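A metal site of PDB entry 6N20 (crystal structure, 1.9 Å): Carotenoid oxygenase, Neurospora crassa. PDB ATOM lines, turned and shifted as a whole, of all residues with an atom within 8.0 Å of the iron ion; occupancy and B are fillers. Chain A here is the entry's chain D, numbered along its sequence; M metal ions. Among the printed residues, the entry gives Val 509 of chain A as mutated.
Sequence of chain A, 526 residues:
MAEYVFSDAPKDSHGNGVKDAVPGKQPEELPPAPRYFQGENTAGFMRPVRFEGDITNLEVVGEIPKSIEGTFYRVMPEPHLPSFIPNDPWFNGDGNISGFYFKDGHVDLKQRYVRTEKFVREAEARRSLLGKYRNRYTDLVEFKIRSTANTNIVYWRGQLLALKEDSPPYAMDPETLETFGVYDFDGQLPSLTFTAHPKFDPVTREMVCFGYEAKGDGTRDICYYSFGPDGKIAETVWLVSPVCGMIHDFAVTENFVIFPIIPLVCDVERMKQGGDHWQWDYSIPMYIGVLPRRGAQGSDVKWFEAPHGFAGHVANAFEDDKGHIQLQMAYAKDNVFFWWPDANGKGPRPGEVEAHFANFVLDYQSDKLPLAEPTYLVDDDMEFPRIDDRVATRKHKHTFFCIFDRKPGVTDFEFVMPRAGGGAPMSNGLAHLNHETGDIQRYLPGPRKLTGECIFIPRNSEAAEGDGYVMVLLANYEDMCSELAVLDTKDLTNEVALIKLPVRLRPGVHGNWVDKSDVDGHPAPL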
ATOM      1  N   THR A 151      -6.921   7.197 -19.321  1.00  0.00           N
ATOM      2  CA  THR A 151      -7.081   5.708 -19.348  1.00  0.00           C
ATOM      3  C   THR A 151      -7.943   5.238 -20.516  1.00  0.00           C
ATOM      4  O   THR A 151      -7.553   4.263 -21.181  1.00  0.00           O
ATOM      5  CB  THR A 151      -7.637   5.191 -18.012  1.00  0.00           C
ATOM      6  OG1 THR A 151      -6.664   5.550 -17.034  1.00  0.00           O
ATOM      7  CG2 THR A 151      -7.807   3.700 -17.990  1.00  0.00           C
ATOM      8  N   ASN A 152      -9.089   5.883 -20.789  1.00  0.00           N
ATOM      9  CA  ASN A 152      -9.970   5.452 -21.901  1.00  0.00           C
ATOM     10  C   ASN A 152     -10.691   6.674 -22.482  1.00  0.00           C
ATOM     11  O   ASN A 152     -10.743   7.727 -21.825  1.00  0.00           O
ATOM     12  CB  ASN A 152     -10.959   4.350 -21.478  1.00  0.00           C
ATOM     13  CG  ASN A 152     -11.477   3.484 -22.612  1.00  0.00           C
ATOM     14  OD1 ASN A 152     -11.223   3.721 -23.798  1.00  0.00           O
ATOM     15  ND2 ASN A 152     -12.244   2.463 -22.260  1.00  0.00           N
ATOM     16  N   GLU A 165     -10.484   6.199 -13.457  1.00  0.00           N
ATOM     17  CA  GLU A 165     -11.382   5.484 -12.508  1.00  0.00           C
ATOM     18  C   GLU A 165     -11.450   6.150 -11.129  1.00  0.00           C
ATOM     19  O   GLU A 165     -12.265   5.682 -10.326  1.00  0.00           O
ATOM     20  CB  GLU A 165     -10.963   4.016 -12.393  1.00  0.00           C
ATOM     21  CG  GLU A 165      -9.603   3.785 -11.763  1.00  0.00           C
ATOM     22  CD  GLU A 165      -9.008   2.433 -12.120  1.00  0.00           C
ATOM     23  OE1 GLU A 165      -8.604   1.698 -11.199  1.00  0.00           O
ATOM     24  OE2 GLU A 165      -8.914   2.137 -13.338  1.00  0.00           O
ATOM     25  N   THR A 195     -15.789   4.275 -13.794  1.00  0.00           N
ATOM     26  CA  THR A 195     -14.866   3.251 -14.343  1.00  0.00           C
ATOM     27  C   THR A 195     -14.326   3.696 -15.709  1.00  0.00           C
ATOM     28  O   THR A 195     -15.070   4.366 -16.481  1.00  0.00           O
ATOM     29  CB  THR A 195     -15.575   1.885 -14.477  1.00  0.00           C
ATOM     30  OG1 THR A 195     -14.606   0.942 -14.927  1.00  0.00           O
ATOM     31  CG2 THR A 195     -16.753   1.921 -15.448  1.00  0.00           C
ATOM     32  N   ALA A 196     -13.094   3.294 -16.020  1.00  0.00           N
ATOM     33  CA  ALA A 196     -12.492   3.447 -17.352  1.00  0.00           C
ATOM     34  C   ALA A 196     -13.063   2.408 -18.327  1.00  0.00           C
ATOM     35  O   ALA A 196     -12.767   2.531 -19.536  1.00  0.00           O
ATOM     36  CB  ALA A 196     -10.991   3.359 -17.273  1.00  0.00           C
ATOM     37  N   HIS A 197     -13.876   1.435 -17.858  1.00  0.00           N
ATOM     38  CA  HIS A 197     -14.362   0.301 -18.686  1.00  0.00           C
ATOM     39  C   HIS A 197     -15.867   0.131 -18.588  1.00  0.00           C
ATOM     40  O   HIS A 197     -16.358  -0.948 -18.250  1.00  0.00           O
ATOM     41  CB  HIS A 197     -13.579  -0.973 -18.332  1.00  0.00           C
ATOM     42  CG  HIS A 197     -12.154  -0.880 -18.752  1.00  0.00           C
ATOM     43  ND1 HIS A 197     -11.814  -0.869 -20.076  1.00  0.00           N
ATOM     44  CD2 HIS A 197     -11.009  -0.704 -18.038  1.00  0.00           C
ATOM     45  CE1 HIS A 197     -10.503  -0.757 -20.165  1.00  0.00           C
ATOM     46  NE2 HIS A 197      -9.970  -0.666 -18.926  1.00  0.00           N
ATOM     47  N   HIS A 248     -10.695  -2.537 -11.664  1.00  0.00           N
ATOM     48  CA  HIS A 248     -10.283  -1.818 -12.891  1.00  0.00           C
ATOM     49  C   HIS A 248     -11.314  -2.053 -13.984  1.00  0.00           C
ATOM     50  O   HIS A 248     -11.635  -1.107 -14.732  1.00  0.00           O
ATOM     51  CB  HIS A 248      -8.893  -2.274 -13.358  1.00  0.00           C
ATOM     52  CG  HIS A 248      -8.473  -1.530 -14.569  1.00  0.00           C
ATOM     53  ND1 HIS A 248      -8.271  -0.152 -14.540  1.00  0.00           N
ATOM     54  CD2 HIS A 248      -8.307  -1.907 -15.869  1.00  0.00           C
ATOM     55  CE1 HIS A 248      -7.983   0.268 -15.759  1.00  0.00           C
ATOM     56  NE2 HIS A 248      -7.998  -0.775 -16.566  1.00  0.00           N
ATOM     57  N   ASP A 249     -11.769  -3.300 -14.121  1.00  0.00           N
ATOM     58  CA  ASP A 249     -12.692  -3.711 -15.207  1.00  0.00           C
ATOM     59  C   ASP A 249     -13.860  -4.469 -14.566  1.00  0.00           C
ATOM     60  O   ASP A 249     -13.752  -4.825 -13.373  1.00  0.00           O
ATOM     61  CB  ASP A 249     -11.921  -4.521 -16.256  1.00  0.00           C
ATOM     62  CG  ASP A 249     -12.527  -4.523 -17.662  1.00  0.00           C
ATOM     63  OD1 ASP A 249     -13.711  -4.128 -17.809  1.00  0.00           O
ATOM     64  OD2 ASP A 249     -11.835  -4.946 -18.590  1.00  0.00           O
ATOM     65  N   GLY A 312      -6.990  -9.217 -14.978  1.00  0.00           N
ATOM     66  CA  GLY A 312      -6.697  -8.388 -16.161  1.00  0.00           C
ATOM     67  C   GLY A 312      -7.976  -7.967 -16.841  1.00  0.00           C
ATOM     68  O   GLY A 312      -9.054  -8.122 -16.228  1.00  0.00           O
ATOM     69  N   HIS A 313      -7.890  -7.481 -18.074  1.00  0.00           N
ATOM     70  CA  HIS A 313      -9.060  -6.924 -18.812  1.00  0.00           C
ATOM     71  C   HIS A 313     -10.039  -8.058 -19.149  1.00  0.00           C
ATOM     72  O   HIS A 313      -9.612  -9.201 -19.453  1.00  0.00           O
ATOM     73  CB  HIS A 313      -8.587  -6.133 -20.030  1.00  0.00           C
ATOM     74  CG  HIS A 313      -7.983  -4.816 -19.661  1.00  0.00           C
ATOM     75  ND1 HIS A 313      -6.618  -4.601 -19.659  1.00  0.00           N
ATOM     76  CD2 HIS A 313      -8.550  -3.659 -19.256  1.00  0.00           C
ATOM     77  CE1 HIS A 313      -6.358  -3.364 -19.269  1.00  0.00           C
ATOM     78  NE2 HIS A 313      -7.536  -2.752 -19.024  1.00  0.00           N
ATOM     79  N   VAL A 314     -11.334  -7.727 -19.075  1.00  0.00           N
ATOM     80  CA  VAL A 314     -12.459  -8.593 -19.508  1.00  0.00           C
ATOM     81  C   VAL A 314     -12.568  -8.533 -21.030  1.00  0.00           C
ATOM     82  O   VAL A 314     -12.614  -7.417 -21.589  1.00  0.00           O
ATOM     83  CB  VAL A 314     -13.769  -8.143 -18.837  1.00  0.00           C
ATOM     84  CG1 VAL A 314     -14.980  -8.859 -19.422  1.00  0.00           C
ATOM     85  CG2 VAL A 314     -13.689  -8.301 -17.325  1.00  0.00           C
ATOM     86  N   PHE A 337       1.005  -5.356 -12.067  1.00  0.00           N
ATOM     87  CA  PHE A 337       1.317  -3.923 -11.770  1.00  0.00           C
ATOM     88  C   PHE A 337       2.421  -3.896 -10.722  1.00  0.00           C
ATOM     89  O   PHE A 337       2.196  -3.405  -9.609  1.00  0.00           O
ATOM     90  CB  PHE A 337       0.059  -3.151 -11.344  1.00  0.00           C
ATOM     91  CG  PHE A 337      -1.042  -3.039 -12.367  1.00  0.00           C
ATOM     92  CD1 PHE A 337      -0.855  -3.370 -13.695  1.00  0.00           C
ATOM     93  CD2 PHE A 337      -2.283  -2.540 -11.985  1.00  0.00           C
ATOM     94  CE1 PHE A 337      -1.891  -3.231 -14.624  1.00  0.00           C
ATOM     95  CE2 PHE A 337      -3.308  -2.391 -12.915  1.00  0.00           C
ATOM     96  CZ  PHE A 337      -3.116  -2.748 -14.231  1.00  0.00           C
ATOM     97  N   GLU A 383      -3.099  -9.821 -23.376  1.00  0.00           N
ATOM     98  CA  GLU A 383      -3.855  -8.748 -22.677  1.00  0.00           C
ATOM     99  C   GLU A 383      -4.585  -7.924 -23.746  1.00  0.00           C
ATOM    100  O   GLU A 383      -4.479  -8.260 -24.937  1.00  0.00           O
ATOM    101  CB  GLU A 383      -2.913  -7.907 -21.795  1.00  0.00           C
ATOM    102  CG  GLU A 383      -3.209  -8.038 -20.291  1.00  0.00           C
ATOM    103  CD  GLU A 383      -4.512  -7.431 -19.810  1.00  0.00           C
ATOM    104  OE1 GLU A 383      -5.199  -6.746 -20.626  1.00  0.00           O
ATOM    105  OE2 GLU A 383      -4.858  -7.620 -18.637  1.00  0.00           O
ATOM    106  N   PHE A 384      -5.339  -6.915 -23.310  1.00  0.00           N
ATOM    107  CA  PHE A 384      -6.084  -5.946 -24.174  1.00  0.00           C
ATOM    108  C   PHE A 384      -7.002  -6.708 -25.131  1.00  0.00           C
ATOM    109  O   PHE A 384      -6.944  -6.487 -26.339  1.00  0.00           O
ATOM    110  CB  PHE A 384      -5.092  -5.020 -24.875  1.00  0.00           C
ATOM    111  CG  PHE A 384      -4.323  -4.142 -23.916  1.00  0.00           C
ATOM    112  CD1 PHE A 384      -4.941  -3.067 -23.301  1.00  0.00           C
ATOM    113  CD2 PHE A 384      -3.003  -4.418 -23.593  1.00  0.00           C
ATOM    114  CE1 PHE A 384      -4.244  -2.279 -22.398  1.00  0.00           C
ATOM    115  CE2 PHE A 384      -2.316  -3.635 -22.665  1.00  0.00           C
ATOM    116  CZ  PHE A 384      -2.950  -2.576 -22.059  1.00  0.00           C
ATOM    117  N   GLU A 453      -3.154  -1.523 -27.948  1.00  0.00           N
ATOM    118  CA  GLU A 453      -4.478  -2.184 -28.029  1.00  0.00           C
ATOM    119  C   GLU A 453      -5.081  -1.961 -29.416  1.00  0.00           C
ATOM    120  O   GLU A 453      -4.989  -0.824 -29.937  1.00  0.00           O
ATOM    121  CB  GLU A 453      -5.400  -1.614 -26.938  1.00  0.00           C
ATOM    122  CG  GLU A 453      -6.783  -2.209 -26.959  1.00  0.00           C
ATOM    123  CD  GLU A 453      -7.801  -1.405 -26.170  1.00  0.00           C
ATOM    124  OE1 GLU A 453      -8.039  -0.238 -26.547  1.00  0.00           O
ATOM    125  OE2 GLU A 453      -8.348  -1.950 -25.156  1.00  0.00           O
ATOM    126  N   VAL A 509      -3.102   3.869 -23.825  1.00  0.00           N
ATOM    127  CA  VAL A 509      -3.907   2.878 -23.068  1.00  0.00           C
ATOM    128  C   VAL A 509      -5.022   2.449 -24.020  1.00  0.00           C
ATOM    129  O   VAL A 509      -4.701   1.838 -25.056  1.00  0.00           O
ATOM    130  CB  VAL A 509      -4.360   3.483 -21.714  1.00  0.00           C
ATOM    131  CG1 VAL A 509      -4.784   2.385 -20.737  1.00  0.00           C
ATOM    132  CG2 VAL A 509      -3.252   4.331 -21.096  1.00  0.00           C
ATOM    133  N   HIS A 510      -6.278   2.805 -23.760  1.00  0.00           N
ATOM    134  CA  HIS A 510      -7.412   2.254 -24.527  1.00  0.00           C
ATOM    135  C   HIS A 510      -7.790   3.204 -25.673  1.00  0.00           C
ATOM    136  O   HIS A 510      -7.383   4.388 -25.663  1.00  0.00           O
ATOM    137  CB  HIS A 510      -8.548   1.928 -23.569  1.00  0.00           C
ATOM    138  CG  HIS A 510      -8.167   0.885 -22.583  1.00  0.00           C
ATOM    139  ND1 HIS A 510      -8.063  -0.448 -22.936  1.00  0.00           N
ATOM    140  CD2 HIS A 510      -7.841   0.965 -21.268  1.00  0.00           C
ATOM    141  CE1 HIS A 510      -7.708  -1.147 -21.855  1.00  0.00           C
ATOM    142  NE2 HIS A 510      -7.546  -0.290 -20.831  1.00  0.00           N
HETATM  143 FE    FE M   1      -7.810  -0.716 -18.699  1.00  0.00          FE
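A ring nitrogen (ND1) of His 248 lies within hydrogen-bond range of the side-chain carboxylate (OE2) of Glu 165 (2.7 Å). The backbone NH (N) of His 197 sits at hydrogen-bond distance from the side-chain hydroxyl (OG1) of Thr 195 (3.1 Å). The side-chain carboxylate of Glu 453 is in hydrogen-bond range of a ring nitrogen (ND1) of His 510 (2.7 Å). O of Thr 151 lies within hydrogen-bond range of N of His 510 (3.2 Å). ND1 of His 313 lies within hydrogen-bond range of OE1 of Glu 383 (2.7 Å).
The iron ion is bound by a ring nitrogen (NE2) of His 313 (2.1 Å), a ring nitrogen (NE2) of His 248 (2.1 Å), a ring nitrogen (NE2) of His 197 (2.2 Å) and a ring nitrogen (NE2) of His 510 (2.2 Å).
Of the 17 residues printed, 4 come within 4 Å of the iron ion. The nearest printed residue that does not touch the iron ion is Thr 151 (4.5 Å).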
